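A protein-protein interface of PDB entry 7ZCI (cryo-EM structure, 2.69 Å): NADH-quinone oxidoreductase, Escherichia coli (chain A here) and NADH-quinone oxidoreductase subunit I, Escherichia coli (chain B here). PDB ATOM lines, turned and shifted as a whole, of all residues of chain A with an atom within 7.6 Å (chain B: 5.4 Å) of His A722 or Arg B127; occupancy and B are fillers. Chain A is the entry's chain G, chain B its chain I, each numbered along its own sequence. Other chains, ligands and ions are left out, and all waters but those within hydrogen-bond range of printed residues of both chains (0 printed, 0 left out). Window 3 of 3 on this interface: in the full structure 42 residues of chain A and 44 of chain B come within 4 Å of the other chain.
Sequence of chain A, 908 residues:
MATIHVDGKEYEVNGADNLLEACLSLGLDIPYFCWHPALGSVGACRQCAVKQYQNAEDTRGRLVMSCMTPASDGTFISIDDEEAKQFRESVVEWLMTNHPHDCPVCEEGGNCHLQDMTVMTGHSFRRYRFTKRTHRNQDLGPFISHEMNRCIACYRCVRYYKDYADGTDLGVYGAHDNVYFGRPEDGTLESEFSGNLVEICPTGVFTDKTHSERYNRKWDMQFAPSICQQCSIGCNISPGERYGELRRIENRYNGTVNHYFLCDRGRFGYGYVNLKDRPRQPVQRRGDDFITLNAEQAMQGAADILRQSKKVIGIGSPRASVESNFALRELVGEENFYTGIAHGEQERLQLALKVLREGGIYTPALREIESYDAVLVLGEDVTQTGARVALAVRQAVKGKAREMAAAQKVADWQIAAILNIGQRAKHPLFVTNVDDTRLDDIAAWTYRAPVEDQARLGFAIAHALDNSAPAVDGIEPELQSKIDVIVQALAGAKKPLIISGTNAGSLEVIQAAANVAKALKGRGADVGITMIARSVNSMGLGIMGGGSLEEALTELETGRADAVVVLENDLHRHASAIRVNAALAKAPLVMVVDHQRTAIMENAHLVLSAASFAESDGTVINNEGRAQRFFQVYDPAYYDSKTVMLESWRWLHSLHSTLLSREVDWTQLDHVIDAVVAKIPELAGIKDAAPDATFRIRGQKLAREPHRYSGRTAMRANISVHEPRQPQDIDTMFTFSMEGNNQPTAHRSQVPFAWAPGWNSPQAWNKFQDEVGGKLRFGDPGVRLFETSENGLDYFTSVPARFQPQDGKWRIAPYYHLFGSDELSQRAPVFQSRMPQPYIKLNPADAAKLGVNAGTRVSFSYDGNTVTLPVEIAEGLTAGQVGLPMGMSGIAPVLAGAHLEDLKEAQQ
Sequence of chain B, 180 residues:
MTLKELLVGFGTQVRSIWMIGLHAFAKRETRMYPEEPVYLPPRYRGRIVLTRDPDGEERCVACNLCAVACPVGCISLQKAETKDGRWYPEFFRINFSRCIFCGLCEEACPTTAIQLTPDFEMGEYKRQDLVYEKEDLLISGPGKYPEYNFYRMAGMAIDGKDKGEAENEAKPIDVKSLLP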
ATOM      1  N   ARG A 712     -21.060 -13.217   7.613  1.00  0.00           N
ATOM      2  CA  ARG A 712     -19.746 -13.478   8.196  1.00  0.00           C
ATOM      3  C   ARG A 712     -19.385 -14.958   8.157  1.00  0.00           C
ATOM      4  O   ARG A 712     -18.225 -15.310   7.923  1.00  0.00           O
ATOM      5  CB  ARG A 712     -19.700 -12.965   9.634  1.00  0.00           C
ATOM      6  CG  ARG A 712     -19.533 -11.461   9.762  1.00  0.00           C
ATOM      7  CD  ARG A 712     -18.596 -11.096  10.911  1.00  0.00           C
ATOM      8  NE  ARG A 712     -17.322 -10.569  10.434  1.00  0.00           N
ATOM      9  CZ  ARG A 712     -16.334 -10.161  11.219  1.00  0.00           C
ATOM     10  NH1 ARG A 712     -16.437 -10.199  12.537  1.00  0.00           N
ATOM     11  NH2 ARG A 712     -15.220  -9.692  10.668  1.00  0.00           N
ATOM     12  N   THR A 713     -20.358 -15.838   8.371  1.00  0.00           N
ATOM     13  CA  THR A 713     -20.101 -17.270   8.368  1.00  0.00           C
ATOM     14  C   THR A 713     -20.496 -17.933   7.059  1.00  0.00           C
ATOM     15  O   THR A 713     -20.579 -19.161   7.002  1.00  0.00           O
ATOM     16  CB  THR A 713     -20.822 -17.948   9.533  1.00  0.00           C
ATOM     17  OG1 THR A 713     -22.233 -17.926   9.311  1.00  0.00           O
ATOM     18  CG2 THR A 713     -20.523 -17.220  10.821  1.00  0.00           C
ATOM     19  N   ARG A 716     -17.324 -16.977   2.731  1.00  0.00           N
ATOM     20  CA  ARG A 716     -16.204 -17.813   2.343  1.00  0.00           C
ATOM     21  C   ARG A 716     -16.507 -19.300   2.475  1.00  0.00           C
ATOM     22  O   ARG A 716     -15.593 -20.118   2.354  1.00  0.00           O
ATOM     23  CB  ARG A 716     -14.982 -17.456   3.183  1.00  0.00           C
ATOM     24  CG  ARG A 716     -13.711 -17.425   2.394  1.00  0.00           C
ATOM     25  CD  ARG A 716     -12.514 -17.390   3.300  1.00  0.00           C
ATOM     26  NE  ARG A 716     -11.346 -17.946   2.632  1.00  0.00           N
ATOM     27  CZ  ARG A 716     -10.675 -19.004   3.058  1.00  0.00           C
ATOM     28  NH1 ARG A 716     -11.020 -19.641   4.163  1.00  0.00           N
ATOM     29  NH2 ARG A 716      -9.637 -19.439   2.353  1.00  0.00           N
ATOM     30  N   ALA A 717     -17.768 -19.668   2.710  1.00  0.00           N
ATOM     31  CA  ALA A 717     -18.101 -21.043   3.060  1.00  0.00           C
ATOM     32  C   ALA A 717     -17.969 -22.005   1.890  1.00  0.00           C
ATOM     33  O   ALA A 717     -17.811 -23.207   2.112  1.00  0.00           O
ATOM     34  CB  ALA A 717     -19.515 -21.110   3.630  1.00  0.00           C
ATOM     35  N   ILE A 719     -15.407 -21.947  -0.092  1.00  0.00           N
ATOM     36  CA  ILE A 719     -13.997 -22.316  -0.041  1.00  0.00           C
ATOM     37  C   ILE A 719     -13.743 -23.269   1.118  1.00  0.00           C
ATOM     38  O   ILE A 719     -13.218 -24.373   0.937  1.00  0.00           O
ATOM     39  CB  ILE A 719     -13.110 -21.062   0.057  1.00  0.00           C
ATOM     40  CG1 ILE A 719     -13.435 -20.079  -1.068  1.00  0.00           C
ATOM     41  CG2 ILE A 719     -11.645 -21.441   0.025  1.00  0.00           C
ATOM     42  CD1 ILE A 719     -13.299 -20.659  -2.447  1.00  0.00           C
ATOM     43  N   SER A 720     -14.113 -22.857   2.325  1.00  0.00           N
ATOM     44  CA  SER A 720     -14.079 -23.739   3.477  1.00  0.00           C
ATOM     45  C   SER A 720     -15.162 -23.308   4.448  1.00  0.00           C
ATOM     46  O   SER A 720     -15.394 -22.113   4.634  1.00  0.00           O
ATOM     47  CB  SER A 720     -12.716 -23.729   4.170  1.00  0.00           C
ATOM     48  OG  SER A 720     -12.746 -24.526   5.337  1.00  0.00           O
ATOM     49  N   VAL A 721     -15.817 -24.291   5.066  1.00  0.00           N
ATOM     50  CA  VAL A 721     -16.868 -24.002   6.030  1.00  0.00           C
ATOM     51  C   VAL A 721     -16.297 -23.434   7.327  1.00  0.00           C
ATOM     52  O   VAL A 721     -17.014 -22.757   8.070  1.00  0.00           O
ATOM     53  CB  VAL A 721     -17.713 -25.276   6.249  1.00  0.00           C
ATOM     54  CG1 VAL A 721     -16.947 -26.316   7.036  1.00  0.00           C
ATOM     55  CG2 VAL A 721     -19.038 -24.952   6.915  1.00  0.00           C
ATOM     56  N   HIS A 722     -15.017 -23.662   7.606  1.00  0.00           N
ATOM     57  CA  HIS A 722     -14.372 -23.077   8.774  1.00  0.00           C
ATOM     58  C   HIS A 722     -14.099 -21.601   8.523  1.00  0.00           C
ATOM     59  O   HIS A 722     -13.409 -21.248   7.561  1.00  0.00           O
ATOM     60  CB  HIS A 722     -13.077 -23.816   9.094  1.00  0.00           C
ATOM     61  CG  HIS A 722     -13.280 -25.255   9.436  1.00  0.00           C
ATOM     62  ND1 HIS A 722     -13.413 -25.699  10.734  1.00  0.00           N
ATOM     63  CD2 HIS A 722     -13.383 -26.353   8.651  1.00  0.00           C
ATOM     64  CE1 HIS A 722     -13.587 -27.007  10.732  1.00  0.00           C
ATOM     65  NE2 HIS A 722     -13.575 -27.428   9.481  1.00  0.00           N
ATOM     66  N   GLU A 723     -14.640 -20.748   9.382  1.00  0.00           N
ATOM     67  CA  GLU A 723     -14.464 -19.310   9.223  1.00  0.00           C
ATOM     68  C   GLU A 723     -13.002 -18.940   9.445  1.00  0.00           C
ATOM     69  O   GLU A 723     -12.412 -19.338  10.454  1.00  0.00           O
ATOM     70  CB  GLU A 723     -15.354 -18.543  10.200  1.00  0.00           C
ATOM     71  CG  GLU A 723     -16.840 -18.692   9.939  1.00  0.00           C
ATOM     72  CD  GLU A 723     -17.437 -19.898  10.641  1.00  0.00           C
ATOM     73  OE1 GLU A 723     -16.789 -20.437  11.560  1.00  0.00           O
ATOM     74  OE2 GLU A 723     -18.546 -20.322  10.262  1.00  0.00           O
ATOM     75  N   PRO A 724     -12.386 -18.202   8.531  1.00  0.00           N
ATOM     76  CA  PRO A 724     -10.973 -17.856   8.681  1.00  0.00           C
ATOM     77  C   PRO A 724     -10.781 -16.791   9.749  1.00  0.00           C
ATOM     78  O   PRO A 724     -11.722 -16.136  10.195  1.00  0.00           O
ATOM     79  CB  PRO A 724     -10.599 -17.326   7.299  1.00  0.00           C
ATOM     80  CG  PRO A 724     -11.851 -16.726   6.806  1.00  0.00           C
ATOM     81  CD  PRO A 724     -12.974 -17.584   7.331  1.00  0.00           C
ATOM     82  N   ARG A 725      -9.527 -16.650  10.165  1.00  0.00           N
ATOM     83  CA  ARG A 725      -9.147 -15.584  11.079  1.00  0.00           C
ATOM     84  C   ARG A 725      -9.397 -14.227  10.433  1.00  0.00           C
ATOM     85  O   ARG A 725      -9.155 -14.040   9.237  1.00  0.00           O
ATOM     86  CB  ARG A 725      -7.673 -15.735  11.457  1.00  0.00           C
ATOM     87  CG  ARG A 725      -7.116 -14.661  12.380  1.00  0.00           C
ATOM     88  CD  ARG A 725      -7.915 -14.535  13.670  1.00  0.00           C
ATOM     89  NE  ARG A 725      -7.614 -13.320  14.425  1.00  0.00           N
ATOM     90  CZ  ARG A 725      -6.474 -13.067  15.057  1.00  0.00           C
ATOM     91  NH1 ARG A 725      -5.475 -13.937  15.068  1.00  0.00           N
ATOM     92  NH2 ARG A 725      -6.339 -11.921  15.720  1.00  0.00           N
ATOM     93  N   ASN B  95     -25.062 -21.538   4.959  1.00  0.00           N
ATOM     94  CA  ASN B  95     -24.277 -22.393   5.844  1.00  0.00           C
ATOM     95  C   ASN B  95     -25.223 -23.033   6.851  1.00  0.00           C
ATOM     96  O   ASN B  95     -25.527 -22.450   7.891  1.00  0.00           O
ATOM     97  CB  ASN B  95     -23.188 -21.580   6.533  1.00  0.00           C
ATOM     98  CG  ASN B  95     -22.117 -22.440   7.176  1.00  0.00           C
ATOM     99  OD1 ASN B  95     -22.243 -23.652   7.276  1.00  0.00           O
ATOM    100  ND2 ASN B  95     -21.054 -21.800   7.621  1.00  0.00           N
ATOM    101  N   SER B  97     -24.634 -25.630   8.698  1.00  0.00           N
ATOM    102  CA  SER B  97     -23.936 -25.922   9.942  1.00  0.00           C
ATOM    103  C   SER B  97     -24.040 -24.772  10.930  1.00  0.00           C
ATOM    104  O   SER B  97     -23.861 -24.980  12.132  1.00  0.00           O
ATOM    105  CB  SER B  97     -22.468 -26.234   9.662  1.00  0.00           C
ATOM    106  OG  SER B  97     -21.767 -25.072   9.273  1.00  0.00           O
ATOM    107  N   ARG B  98     -24.321 -23.567  10.446  1.00  0.00           N
ATOM    108  CA  ARG B  98     -24.458 -22.388  11.281  1.00  0.00           C
ATOM    109  C   ARG B  98     -25.901 -22.006  11.550  1.00  0.00           C
ATOM    110  O   ARG B  98     -26.179 -21.393  12.581  1.00  0.00           O
ATOM    111  CB  ARG B  98     -23.749 -21.205  10.623  1.00  0.00           C
ATOM    112  CG  ARG B  98     -22.278 -21.133  10.897  1.00  0.00           C
ATOM    113  CD  ARG B  98     -22.024 -20.373  12.165  1.00  0.00           C
ATOM    114  NE  ARG B  98     -20.605 -20.287  12.475  1.00  0.00           N
ATOM    115  CZ  ARG B  98     -20.117 -19.769  13.590  1.00  0.00           C
ATOM    116  NH1 ARG B  98     -20.908 -19.281  14.526  1.00  0.00           N
ATOM    117  NH2 ARG B  98     -18.803 -19.738  13.768  1.00  0.00           N
ATOM    118  N   TYR B 125     -22.367 -36.087   6.606  1.00  0.00           N
ATOM    119  CA  TYR B 125     -21.106 -36.725   6.956  1.00  0.00           C
ATOM    120  C   TYR B 125     -19.969 -35.726   7.087  1.00  0.00           C
ATOM    121  O   TYR B 125     -19.158 -35.826   8.010  1.00  0.00           O
ATOM    122  CB  TYR B 125     -20.744 -37.772   5.909  1.00  0.00           C
ATOM    123  CG  TYR B 125     -21.609 -38.999   5.951  1.00  0.00           C
ATOM    124  CD1 TYR B 125     -22.330 -39.398   4.839  1.00  0.00           C
ATOM    125  CD2 TYR B 125     -21.697 -39.767   7.100  1.00  0.00           C
ATOM    126  CE1 TYR B 125     -23.120 -40.520   4.874  1.00  0.00           C
ATOM    127  CE2 TYR B 125     -22.483 -40.892   7.142  1.00  0.00           C
ATOM    128  CZ  TYR B 125     -23.190 -41.265   6.027  1.00  0.00           C
ATOM    129  OH  TYR B 125     -23.977 -42.388   6.064  1.00  0.00           O
ATOM    130  N   LYS B 126     -19.882 -34.772   6.169  1.00  0.00           N
ATOM    131  CA  LYS B 126     -18.864 -33.737   6.200  1.00  0.00           C
ATOM    132  C   LYS B 126     -19.530 -32.380   6.347  1.00  0.00           C
ATOM    133  O   LYS B 126     -20.550 -32.111   5.712  1.00  0.00           O
ATOM    134  CB  LYS B 126     -18.015 -33.766   4.934  1.00  0.00           C
ATOM    135  CG  LYS B 126     -17.603 -35.155   4.509  1.00  0.00           C
ATOM    136  CD  LYS B 126     -16.120 -35.225   4.246  1.00  0.00           C
ATOM    137  CE  LYS B 126     -15.349 -35.401   5.536  1.00  0.00           C
ATOM    138  NZ  LYS B 126     -15.686 -36.678   6.211  1.00  0.00           N
ATOM    139  N   ARG B 127     -18.943 -31.529   7.189  1.00  0.00           N
ATOM    140  CA  ARG B 127     -19.512 -30.216   7.460  1.00  0.00           C
ATOM    141  C   ARG B 127     -19.491 -29.306   6.243  1.00  0.00           C
ATOM    142  O   ARG B 127     -20.315 -28.393   6.162  1.00  0.00           O
ATOM    143  CB  ARG B 127     -18.765 -29.556   8.615  1.00  0.00           C
ATOM    144  CG  ARG B 127     -19.603 -28.599   9.423  1.00  0.00           C
ATOM    145  CD  ARG B 127     -18.784 -27.960  10.521  1.00  0.00           C
ATOM    146  NE  ARG B 127     -18.670 -26.520  10.342  1.00  0.00           N
ATOM    147  CZ  ARG B 127     -17.829 -25.747  11.009  1.00  0.00           C
ATOM    148  NH1 ARG B 127     -16.983 -26.246  11.891  1.00  0.00           N
ATOM    149  NH2 ARG B 127     -17.845 -24.438  10.792  1.00  0.00           N
ATOM    150  N   GLN B 128     -18.569 -29.529   5.304  1.00  0.00           N
ATOM    151  CA  GLN B 128     -18.552 -28.760   4.065  1.00  0.00           C
ATOM    152  C   GLN B 128     -19.801 -29.011   3.233  1.00  0.00           C
ATOM    153  O   GLN B 128     -20.271 -28.108   2.533  1.00  0.00           O
ATOM    154  CB  GLN B 128     -17.295 -29.099   3.260  1.00  0.00           C
ATOM    155  CG  GLN B 128     -17.057 -28.231   2.030  1.00  0.00           C
ATOM    156  CD  GLN B 128     -16.885 -26.764   2.360  1.00  0.00           C
ATOM    157  OE1 GLN B 128     -16.150 -26.406   3.271  1.00  0.00           O
ATOM    158  NE2 GLN B 128     -17.569 -25.907   1.618  1.00  0.00           N
ATOM    159  N   ASP B 129     -20.371 -30.209   3.319  1.00  0.00           N
ATOM    160  CA  ASP B 129     -21.597 -30.539   2.604  1.00  0.00           C
ATOM    161  C   ASP B 129     -22.834 -29.896   3.207  1.00  0.00           C
ATOM    162  O   ASP B 129     -23.920 -30.050   2.647  1.00  0.00           O
ATOM    163  CB  ASP B 129     -21.775 -32.051   2.554  1.00  0.00           C
ATOM    164  CG  ASP B 129     -20.675 -32.734   1.789  1.00  0.00           C
ATOM    165  OD1 ASP B 129     -20.168 -32.135   0.822  1.00  0.00           O
ATOM    166  OD2 ASP B 129     -20.313 -33.870   2.151  1.00  0.00           O
ATOM    167  N   LEU B 130     -22.707 -29.196   4.327  1.00  0.00           N
ATOM    168  CA  LEU B 130     -23.796 -28.420   4.889  1.00  0.00           C
ATOM    169  C   LEU B 130     -23.865 -27.011   4.321  1.00  0.00           C
ATOM    170  O   LEU B 130     -24.719 -26.229   4.743  1.00  0.00           O
ATOM    171  CB  LEU B 130     -23.665 -28.362   6.411  1.00  0.00           C
ATOM    172  CG  LEU B 130     -24.251 -29.560   7.146  1.00  0.00           C
ATOM    173  CD1 LEU B 130     -24.022 -29.441   8.634  1.00  0.00           C
ATOM    174  CD2 LEU B 130     -25.725 -29.683   6.837  1.00  0.00           C
ATOM    175  N   VAL B 131     -22.984 -26.655   3.392  1.00  0.00           N
ATOM    176  CA  VAL B 131     -23.096 -25.389   2.678  1.00  0.00           C
ATOM    177  C   VAL B 131     -23.911 -25.661   1.420  1.00  0.00           C
ATOM    178  O   VAL B 131     -23.451 -26.343   0.505  1.00  0.00           O
ATOM    179  CB  VAL B 131     -21.726 -24.790   2.342  1.00  0.00           C
ATOM    180  CG1 VAL B 131     -21.897 -23.402   1.754  1.00  0.00           C
ATOM    181  CG2 VAL B 131     -20.853 -24.737   3.572  1.00  0.00           C
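Among the printed residues, merely in contact across the chains: Ser A720 with Gln B128, Val A721 with Asn B95, Thr A713 with Arg B98, Val A721 with Ser B97, His A722 with Arg B127, Ala A717 with Val B131, Val A721 with Val B131 and Glu A723 with Asn B95.
The side-chain hydroxyl of Ser B97 sits at hydrogen-bond distance from the side-chain amide oxygen of Asn B95, at 2.5 Å. OG of Ser A720 lies close to N of His A722.
Of the 11 printed residues of chain A, 6 touch a printed residue of chain B. Hydrophobic or aromatic side chains of chain A that line the printed part of chain B: Ala A717, Val A721 and His A722. Of the 10 printed residues of chain B, 6 touch a printed residue of chain A. Printed residues of chain B that touch a printed residue of chain A: Asn B95, Ser B97, Arg B98, Arg B127, Gln B128 and Val B131. Hydrophobic or aromatic side chains of chain B within 4 Å of the printed part of chain A: Val B131.
NH2 of Arg B127 lies within hydrogen-bond range of O of Val A721, 3.3 Å away. NE of Arg B98 lies within salt-bridge range of OE2 of Glu A723, at 3.0 Å. N of Val A721 is in hydrogen-bond range of OE1 of Gln B128 (2.8 Å). O of Ala A717 is in hydrogen-bond range of NE2 of Gln B128, 2.8 Å away. The backbone carbonyl oxygen (O) of Thr A713 lies within hydrogen-bond range of the side-chain amide nitrogen (ND2) of Asn B95, 2.8 Å away.
Arg B127 touches just these residues of chain A: Val A721 and His A722. Of the printed residues of chain B, Glu A723 touches Asn B95 (3.9 Å) and Arg B98 (3.0 Å). Printed residues of chain A within 4 Å of Arg B98: Thr A713 and Glu A723. Printed residues of chain A within 4 Å of Gln B128: Ala A717 (2.8 Å), Ser A720 (3.4 Å) and Val A721 (2.8 Å). Printed residues of chain B within 4 Å of Ala A717: Gln B128 (2.8 Å) and Val B131 (3.7 Å). Arg A712 touches none of the printed residues of chain B. Ile A719 touches none of the printed residues of chain B. The nearest residue of chain B that does not touch His A722 is Gln B128 (5.3 Å). The nearest residue of chain A that does not touch Arg B127 is Glu A723 (4.2 Å).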
